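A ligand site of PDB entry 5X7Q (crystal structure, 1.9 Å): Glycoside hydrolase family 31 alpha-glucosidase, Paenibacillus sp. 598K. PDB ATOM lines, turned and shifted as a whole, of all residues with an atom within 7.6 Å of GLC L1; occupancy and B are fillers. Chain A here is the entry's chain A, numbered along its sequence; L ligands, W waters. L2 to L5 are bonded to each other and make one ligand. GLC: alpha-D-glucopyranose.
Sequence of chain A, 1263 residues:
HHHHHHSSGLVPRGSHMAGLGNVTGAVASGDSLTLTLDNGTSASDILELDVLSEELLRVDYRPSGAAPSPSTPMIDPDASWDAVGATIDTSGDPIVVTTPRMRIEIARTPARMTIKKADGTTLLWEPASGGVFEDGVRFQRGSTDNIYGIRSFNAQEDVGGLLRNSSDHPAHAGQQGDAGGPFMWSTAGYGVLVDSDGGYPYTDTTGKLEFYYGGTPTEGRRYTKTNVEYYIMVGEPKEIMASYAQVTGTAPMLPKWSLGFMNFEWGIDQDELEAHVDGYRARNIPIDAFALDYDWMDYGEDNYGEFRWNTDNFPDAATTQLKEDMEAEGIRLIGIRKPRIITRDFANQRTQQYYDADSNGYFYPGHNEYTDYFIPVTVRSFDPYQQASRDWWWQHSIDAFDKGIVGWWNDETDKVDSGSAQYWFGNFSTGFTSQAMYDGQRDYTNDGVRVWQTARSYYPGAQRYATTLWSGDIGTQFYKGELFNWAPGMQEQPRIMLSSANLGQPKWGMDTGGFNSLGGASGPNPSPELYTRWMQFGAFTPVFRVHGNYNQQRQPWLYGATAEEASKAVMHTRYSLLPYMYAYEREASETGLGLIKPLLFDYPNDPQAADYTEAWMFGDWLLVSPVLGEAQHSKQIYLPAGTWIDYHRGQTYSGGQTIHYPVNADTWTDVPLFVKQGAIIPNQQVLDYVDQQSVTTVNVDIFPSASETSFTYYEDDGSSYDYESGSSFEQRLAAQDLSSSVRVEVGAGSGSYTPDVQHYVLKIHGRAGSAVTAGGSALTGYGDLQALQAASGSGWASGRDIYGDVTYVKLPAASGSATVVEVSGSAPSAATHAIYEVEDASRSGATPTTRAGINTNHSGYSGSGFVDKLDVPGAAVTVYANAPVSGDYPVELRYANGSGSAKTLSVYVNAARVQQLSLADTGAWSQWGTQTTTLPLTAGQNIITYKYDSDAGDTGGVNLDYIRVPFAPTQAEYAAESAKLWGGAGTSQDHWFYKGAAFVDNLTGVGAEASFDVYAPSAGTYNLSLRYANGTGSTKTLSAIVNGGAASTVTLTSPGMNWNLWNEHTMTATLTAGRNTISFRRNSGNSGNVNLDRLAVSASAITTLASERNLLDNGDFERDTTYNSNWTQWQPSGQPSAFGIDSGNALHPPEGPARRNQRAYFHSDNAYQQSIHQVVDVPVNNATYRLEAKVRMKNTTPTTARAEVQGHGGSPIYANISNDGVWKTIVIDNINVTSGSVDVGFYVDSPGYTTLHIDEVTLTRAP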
ATOM      1  N   SER A 988      15.940   5.559  17.422  1.00  0.00           N
ATOM      2  CA  SER A 988      15.070   6.433  18.182  1.00  0.00           C
ATOM      3  C   SER A 988      13.652   5.853  18.268  1.00  0.00           C
ATOM      4  O   SER A 988      13.255   5.010  17.443  1.00  0.00           O
ATOM      5  CB  SER A 988      15.024   7.808  17.532  1.00  0.00           C
ATOM      6  OG  SER A 988      14.182   8.713  18.256  1.00  0.00           O
ATOM      7  N   ASP A 990      11.288   8.471  19.086  1.00  0.00           N
ATOM      8  CA  ASP A 990      10.658   9.794  19.336  1.00  0.00           C
ATOM      9  C   ASP A 990       9.684  10.277  18.242  1.00  0.00           C
ATOM     10  O   ASP A 990       9.382  11.457  18.155  1.00  0.00           O
ATOM     11  CB  ASP A 990      11.735  10.849  19.664  1.00  0.00           C
ATOM     12  CG  ASP A 990      12.429  11.401  18.432  1.00  0.00           C
ATOM     13  OD1 ASP A 990      12.430  10.759  17.356  1.00  0.00           O
ATOM     14  OD2 ASP A 990      12.954  12.527  18.550  1.00  0.00           O
ATOM     15  N   HIS A 991       9.206   9.353  17.411  1.00  0.00           N
ATOM     16  CA  HIS A 991       8.069   9.608  16.520  1.00  0.00           C
ATOM     17  C   HIS A 991       7.175   8.377  16.573  1.00  0.00           C
ATOM     18  O   HIS A 991       7.600   7.316  17.053  1.00  0.00           O
ATOM     19  CB  HIS A 991       8.524   9.887  15.078  1.00  0.00           C
ATOM     20  CG  HIS A 991       9.346  11.143  14.939  1.00  0.00           C
ATOM     21  ND1 HIS A 991       8.853  12.388  15.254  1.00  0.00           N
ATOM     22  CD2 HIS A 991      10.629  11.327  14.525  1.00  0.00           C
ATOM     23  CE1 HIS A 991       9.791  13.296  15.041  1.00  0.00           C
ATOM     24  NE2 HIS A 991      10.875  12.678  14.596  1.00  0.00           N
ATOM     25  N   PHE A 999      13.260   2.966  15.138  1.00  0.00           N
ATOM     26  CA  PHE A 999      13.606   3.305  13.772  1.00  0.00           C
ATOM     27  C   PHE A 999      14.974   3.998  13.758  1.00  0.00           C
ATOM     28  O   PHE A 999      15.534   4.300  14.827  1.00  0.00           O
ATOM     29  CB  PHE A 999      12.538   4.204  13.130  1.00  0.00           C
ATOM     30  CG  PHE A 999      12.309   5.492  13.848  1.00  0.00           C
ATOM     31  CD1 PHE A 999      13.043   6.634  13.524  1.00  0.00           C
ATOM     32  CD2 PHE A 999      11.339   5.571  14.839  1.00  0.00           C
ATOM     33  CE1 PHE A 999      12.845   7.822  14.209  1.00  0.00           C
ATOM     34  CE2 PHE A 999      11.129   6.755  15.528  1.00  0.00           C
ATOM     35  CZ  PHE A 999      11.878   7.883  15.217  1.00  0.00           C
ATOM     36  N   VAL A1000      15.499   4.242  12.554  1.00  0.00           N
ATOM     37  CA  VAL A1000      16.786   4.930  12.370  1.00  0.00           C
ATOM     38  C   VAL A1000      16.570   6.424  12.016  1.00  0.00           C
ATOM     39  O   VAL A1000      15.788   6.752  11.126  1.00  0.00           O
ATOM     40  CB  VAL A1000      17.619   4.224  11.301  1.00  0.00           C
ATOM     41  CG1 VAL A1000      18.840   5.051  10.906  1.00  0.00           C
ATOM     42  CG2 VAL A1000      18.045   2.838  11.798  1.00  0.00           C
ATOM     43  N   ASP A1001      17.272   7.316  12.718  1.00  0.00           N
ATOM     44  CA  ASP A1001      17.223   8.753  12.461  1.00  0.00           C
ATOM     45  C   ASP A1001      18.644   9.330  12.311  1.00  0.00           C
ATOM     46  O   ASP A1001      19.608   8.567  12.184  1.00  0.00           O
ATOM     47  CB  ASP A1001      16.411   9.482  13.551  1.00  0.00           C
ATOM     48  CG  ASP A1001      17.140   9.568  14.911  1.00  0.00           C
ATOM     49  OD1 ASP A1001      18.177   8.909  15.165  1.00  0.00           O
ATOM     50  OD2 ASP A1001      16.625  10.311  15.752  1.00  0.00           O
ATOM     51  N   ASN A1002      18.752  10.661  12.308  1.00  0.00           N
ATOM     52  CA  ASN A1002      20.061  11.342  12.252  1.00  0.00           C
ATOM     53  C   ASN A1002      20.869  10.913  11.016  1.00  0.00           C
ATOM     54  O   ASN A1002      22.068  10.625  11.093  1.00  0.00           O
ATOM     55  CB  ASN A1002      20.831  11.111  13.578  1.00  0.00           C
ATOM     56  CG  ASN A1002      21.714  12.302  13.976  1.00  0.00           C
ATOM     57  OD1 ASN A1002      21.246  13.427  14.021  1.00  0.00           O
ATOM     58  ND2 ASN A1002      22.981  12.042  14.270  1.00  0.00           N
ATOM     59  N   LEU A1003      20.188  10.837   9.861  1.00  0.00           N
ATOM     60  CA  LEU A1003      20.869  10.673   8.568  1.00  0.00           C
ATOM     61  C   LEU A1003      21.149  12.067   7.983  1.00  0.00           C
ATOM     62  O   LEU A1003      20.690  12.423   6.910  1.00  0.00           O
ATOM     63  CB  LEU A1003      20.032   9.822   7.623  1.00  0.00           C
ATOM     64  CG  LEU A1003      19.830   8.364   8.052  1.00  0.00           C
ATOM     65  CD1 LEU A1003      18.774   7.692   7.195  1.00  0.00           C
ATOM     66  CD2 LEU A1003      21.137   7.583   7.979  1.00  0.00           C
ATOM     67  N   THR A1004      21.919  12.850   8.736  1.00  0.00           N
ATOM     68  CA  THR A1004      22.081  14.270   8.516  1.00  0.00           C
ATOM     69  C   THR A1004      23.451  14.595   7.937  1.00  0.00           C
ATOM     70  O   THR A1004      23.555  15.362   6.992  1.00  0.00           O
ATOM     71  CB  THR A1004      21.891  15.031   9.836  1.00  0.00           C
ATOM     72  OG1 THR A1004      22.688  14.422  10.843  1.00  0.00           O
ATOM     73  CG2 THR A1004      20.448  15.003  10.267  1.00  0.00           C
ATOM     74  N   ALA A1029      10.294   7.698   6.658  1.00  0.00           N
ATOM     75  CA  ALA A1029       9.543   8.911   6.958  1.00  0.00           C
ATOM     76  C   ALA A1029      10.340  10.092   6.423  1.00  0.00           C
ATOM     77  O   ALA A1029      11.589  10.093   6.458  1.00  0.00           O
ATOM     78  CB  ALA A1029       9.329   9.055   8.452  1.00  0.00           C
ATOM     79  N   GLY A1031       9.348  14.059   6.947  1.00  0.00           N
ATOM     80  CA  GLY A1031       8.485  15.147   7.419  1.00  0.00           C
ATOM     81  C   GLY A1031       9.073  16.537   7.238  1.00  0.00           C
ATOM     82  O   GLY A1031       8.687  17.467   7.937  1.00  0.00           O
ATOM     83  N   THR A1032      10.003  16.684   6.290  1.00  0.00           N
ATOM     84  CA  THR A1032      10.619  17.980   6.000  1.00  0.00           C
ATOM     85  C   THR A1032       9.699  18.890   5.179  1.00  0.00           C
ATOM     86  O   THR A1032       9.875  20.108   5.186  1.00  0.00           O
ATOM     87  CB  THR A1032      11.960  17.825   5.250  1.00  0.00           C
ATOM     88  OG1 THR A1032      11.726  17.247   3.954  1.00  0.00           O
ATOM     89  CG2 THR A1032      12.918  16.943   6.036  1.00  0.00           C
ATOM     90  N   LYS A1036      13.615  14.385  -0.567  1.00  0.00           N
ATOM     91  CA  LYS A1036      14.984  14.221  -0.083  1.00  0.00           C
ATOM     92  C   LYS A1036      15.573  13.020  -0.764  1.00  0.00           C
ATOM     93  O   LYS A1036      14.852  12.241  -1.385  1.00  0.00           O
ATOM     94  CB  LYS A1036      15.001  14.015   1.443  1.00  0.00           C
ATOM     95  CG  LYS A1036      14.625  15.238   2.263  1.00  0.00           C
ATOM     96  CD  LYS A1036      15.682  16.342   2.183  1.00  0.00           C
ATOM     97  CE  LYS A1036      15.238  17.618   2.875  1.00  0.00           C
ATOM     98  NZ  LYS A1036      14.005  18.194   2.256  1.00  0.00           N
ATOM     99  N   TRP A1059       6.239  13.777  10.919  1.00  0.00           N
ATOM    100  CA  TRP A1059       7.193  12.671  11.049  1.00  0.00           C
ATOM    101  C   TRP A1059       6.550  11.338  11.514  1.00  0.00           C
ATOM    102  O   TRP A1059       7.239  10.321  11.600  1.00  0.00           O
ATOM    103  CB  TRP A1059       8.341  13.077  11.977  1.00  0.00           C
ATOM    104  CG  TRP A1059       9.281  14.059  11.356  1.00  0.00           C
ATOM    105  CD1 TRP A1059       9.316  15.422  11.552  1.00  0.00           C
ATOM    106  CD2 TRP A1059      10.342  13.759  10.431  1.00  0.00           C
ATOM    107  NE1 TRP A1059      10.337  15.975  10.816  1.00  0.00           N
ATOM    108  CE2 TRP A1059      10.973  14.989  10.109  1.00  0.00           C
ATOM    109  CE3 TRP A1059      10.811  12.572   9.844  1.00  0.00           C
ATOM    110  CZ2 TRP A1059      12.062  15.058   9.224  1.00  0.00           C
ATOM    111  CZ3 TRP A1059      11.892  12.648   8.968  1.00  0.00           C
ATOM    112  CH2 TRP A1059      12.502  13.881   8.658  1.00  0.00           C
ATOM    113  N   SER A1087      20.678  14.920  -0.011  1.00  0.00           N
ATOM    114  CA  SER A1087      20.158  15.792   1.030  1.00  0.00           C
ATOM    115  C   SER A1087      19.952  15.092   2.379  1.00  0.00           C
ATOM    116  O   SER A1087      19.960  15.746   3.407  1.00  0.00           O
ATOM    117  CB  SER A1087      18.833  16.426   0.561  1.00  0.00           C
ATOM    118  OG  SER A1087      18.009  15.429  -0.049  1.00  0.00           O
ATOM    119  N   GLY A1088      19.729  13.774   2.389  1.00  0.00           N
ATOM    120  CA  GLY A1088      19.490  13.039   3.636  1.00  0.00           C
ATOM    121  C   GLY A1088      18.248  13.497   4.377  1.00  0.00           C
ATOM    122  O   GLY A1088      17.252  13.824   3.755  1.00  0.00           O
ATOM    123  N   ASN A1089      18.331  13.524   5.709  1.00  0.00           N
ATOM    124  CA  ASN A1089      17.265  14.042   6.581  1.00  0.00           C
ATOM    125  C   ASN A1089      15.940  13.304   6.414  1.00  0.00           C
ATOM    126  O   ASN A1089      14.881  13.907   6.288  1.00  0.00           O
ATOM    127  CB  ASN A1089      17.095  15.564   6.415  1.00  0.00           C
ATOM    128  CG  ASN A1089      18.314  16.328   6.902  1.00  0.00           C
ATOM    129  OD1 ASN A1089      18.327  16.814   8.020  1.00  0.00           O
ATOM    130  ND2 ASN A1089      19.348  16.383   6.092  1.00  0.00           N
ATOM    131  N   VAL A1090      16.056  11.975   6.403  1.00  0.00           N
ATOM    132  CA  VAL A1090      14.910  11.052   6.441  1.00  0.00           C
ATOM    133  C   VAL A1090      15.160  10.047   7.558  1.00  0.00           C
ATOM    134  O   VAL A1090      16.290   9.895   8.042  1.00  0.00           O
ATOM    135  CB  VAL A1090      14.676  10.305   5.107  1.00  0.00           C
ATOM    136  CG1 VAL A1090      14.287  11.275   3.996  1.00  0.00           C
ATOM    137  CG2 VAL A1090      15.896   9.487   4.684  1.00  0.00           C
ATOM    138  N   ASN A1091      14.090   9.376   7.968  1.00  0.00           N
ATOM    139  CA  ASN A1091      14.166   8.289   8.930  1.00  0.00           C
ATOM    140  C   ASN A1091      13.860   6.993   8.209  1.00  0.00           C
ATOM    141  O   ASN A1091      13.002   6.972   7.330  1.00  0.00           O
ATOM    142  CB  ASN A1091      13.203   8.545  10.104  1.00  0.00           C
ATOM    143  CG  ASN A1091      13.513   9.806  10.859  1.00  0.00           C
ATOM    144  OD1 ASN A1091      14.658  10.286  10.868  1.00  0.00           O
ATOM    145  ND2 ASN A1091      12.492  10.371  11.518  1.00  0.00           N
HETATM  146  C1  GLC L   1      13.879  16.219  13.116  1.00  0.00           C
HETATM  147  C2  GLC L   1      13.193  14.871  13.399  1.00  0.00           C
HETATM  148  C3  GLC L   1      14.124  13.656  13.229  1.00  0.00           C
HETATM  149  C4  GLC L   1      14.897  13.707  11.906  1.00  0.00           C
HETATM  150  C5  GLC L   1      15.538  15.089  11.711  1.00  0.00           C
HETATM  151  C6  GLC L   1      16.174  15.221  10.332  1.00  0.00           C
HETATM  152  O1  GLC L   1      14.796  16.597  14.162  1.00  0.00           O
HETATM  153  O2  GLC L   1      12.688  14.872  14.740  1.00  0.00           O
HETATM  154  O3  GLC L   1      13.358  12.463  13.298  1.00  0.00           O
HETATM  155  O4  GLC L   1      15.914  12.690  11.860  1.00  0.00           O
HETATM  156  O5  GLC L   1      14.563  16.138  11.858  1.00  0.00           O
HETATM  157  O6  GLC L   1      16.769  16.515  10.215  1.00  0.00           O
HETATM  158  C1  GLC L   2       5.522  22.092  11.732  1.00  0.00           C
HETATM  159  C2  GLC L   2       4.156  21.800  11.118  1.00  0.00           C
HETATM  160  C3  GLC L   2       3.319  20.906  12.027  1.00  0.00           C
HETATM  161  C4  GLC L   2       4.076  19.647  12.422  1.00  0.00           C
HETATM  162  C5  GLC L   2       5.513  19.934  12.903  1.00  0.00           C
HETATM  163  C6  GLC L   2       6.311  18.635  13.010  1.00  0.00           C
HETATM  164  O1  GLC L   2       5.378  22.868  12.937  1.00  0.00           O
HETATM  165  O2  GLC L   2       3.439  23.023  10.890  1.00  0.00           O
HETATM  166  O3  GLC L   2       2.112  20.523  11.353  1.00  0.00           O
HETATM  167  O4  GLC L   2       3.312  18.944  13.427  1.00  0.00           O
HETATM  168  O5  GLC L   2       6.187  20.861  12.022  1.00  0.00           O
HETATM  169  O6  GLC L   2       7.569  18.709  12.318  1.00  0.00           O
HETATM  170  C1  GLC L   3       2.715  17.718  12.968  1.00  0.00           C
HETATM  171  C2  GLC L   3       1.467  17.425  13.809  1.00  0.00           C
HETATM  172  C3  GLC L   3       1.848  17.111  15.248  1.00  0.00           C
HETATM  173  C4  GLC L   3       2.872  15.978  15.306  1.00  0.00           C
HETATM  174  C5  GLC L   3       4.056  16.241  14.344  1.00  0.00           C
HETATM  175  C6  GLC L   3       4.982  15.041  14.201  1.00  0.00           C
HETATM  176  O2  GLC L   3       0.589  18.561  13.757  1.00  0.00           O
HETATM  177  O3  GLC L   3       0.685  16.728  15.995  1.00  0.00           O
HETATM  178  O4  GLC L   3       3.321  15.846  16.664  1.00  0.00           O
HETATM  179  O5  GLC L   3       3.594  16.586  13.030  1.00  0.00           O
HETATM  180  O6  GLC L   3       6.075  15.307  13.311  1.00  0.00           O
HETATM  181  C1  GLC L   4       2.884  14.649  17.369  1.00  0.00           C
HETATM  182  C2  GLC L   4       2.649  15.005  18.834  1.00  0.00           C
HETATM  183  C3  GLC L   4       3.946  15.350  19.554  1.00  0.00           C
HETATM  184  C4  GLC L   4       5.040  14.313  19.348  1.00  0.00           C
HETATM  185  C5  GLC L   4       5.121  13.890  17.879  1.00  0.00           C
HETATM  186  C6  GLC L   4       6.105  12.737  17.661  1.00  0.00           C
HETATM  187  O2  GLC L   4       1.766  16.121  18.906  1.00  0.00           O
HETATM  188  O3  GLC L   4       3.713  15.469  20.963  1.00  0.00           O
HETATM  189  O4  GLC L   4       6.263  14.995  19.662  1.00  0.00           O
HETATM  190  O5  GLC L   4       3.825  13.566  17.333  1.00  0.00           O
HETATM  191  O6  GLC L   4       6.319  12.602  16.249  1.00  0.00           O
HETATM  192  C1  GLC L   5       6.994  14.642  20.843  1.00  0.00           C
HETATM  193  C2  GLC L   5       7.120  15.820  21.816  1.00  0.00           C
HETATM  194  C3  GLC L   5       7.861  16.982  21.133  1.00  0.00           C
HETATM  195  C4  GLC L   5       9.222  16.522  20.625  1.00  0.00           C
HETATM  196  C5  GLC L   5       9.115  15.237  19.793  1.00  0.00           C
HETATM  197  C6  GLC L   5      10.489  14.639  19.490  1.00  0.00           C
HETATM  198  O2  GLC L   5       5.835  16.249  22.284  1.00  0.00           O
HETATM  199  O3  GLC L   5       8.015  18.071  22.038  1.00  0.00           O
HETATM  200  O4  GLC L   5       9.834  17.564  19.838  1.00  0.00           O
HETATM  201  O5  GLC L   5       8.316  14.232  20.470  1.00  0.00           O
HETATM  202  O6  GLC L   5      10.456  14.064  18.182  1.00  0.00           O
HETATM  203  O   HOH W   1      17.437  11.815   9.500  1.00  0.00           O
HETATM  204  O   HOH W   2      13.910  13.963  16.708  1.00  0.00           O
HETATM  205  O   HOH W   3      14.132  11.165  15.459  1.00  0.00           O
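Water W2 lies within hydrogen-bond range of an oxygen (O2) of GLC L1 and the side-chain carboxylate of Asp 990.
Water W3 lies within hydrogen-bond range of the side-chain carboxylate (OD1) of Asp 990 (2.6 Å), an oxygen (O3) of GLC L1 (2.6 Å) and the side-chain carboxylate (OD2) of Asp 1001 (2.7 Å).
Water W1 lies within hydrogen-bond range of O of Val 1090 (2.7 Å), O4 of GLC L1 (2.9 Å), N of Leu 1003 (2.9 Å), N of Asn 1002 (3.3 Å) and OD1 of Asn 1091 (3.5 Å).
The backbone carbonyl oxygen (O) of Leu 1003 is in hydrogen-bond range of the backbone NH (N) of Asn 1089, 2.9 Å away.
O of Asn 1091 is in hydrogen-bond range of N of Ala 1029 (2.9 Å).
O of Ser 1087 sits at hydrogen-bond distance from ND2 of Asn 1089 (2.8 Å).
A ring nitrogen (NE2) of His 991 lies within hydrogen-bond range of an oxygen (O3) of GLC L1 (2.8 Å).
An oxygen (O6) of GLC L1 lies within hydrogen-bond range of the side-chain amide oxygen (OD1) of Asn 1089, 2.7 Å away.
The backbone carbonyl oxygen (O) of Asp 990 is in hydrogen-bond range of an oxygen (O6) of GLC L5, 2.8 Å away.
ND2 of Asn 1091 sits at hydrogen-bond distance from O3 of GLC L1.
An oxygen (O6) of GLC L5 sits at hydrogen-bond distance from the side-chain carboxylate (OD2) of Asp 990, 3.0 Å away.
N of Trp 1059 is in hydrogen-bond range of O6 of GLC L3.
O6 of GLC L4 is in hydrogen-bond range of ND1 of His 991 (2.7 Å).
Merely in contact with GLC L1: Asn 1002, Asp 1001, Trp 1059 and Thr 1004.
Hydrophobic or aromatic side chains within 4 Å of GLC L1: His 991 and Trp 1059.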
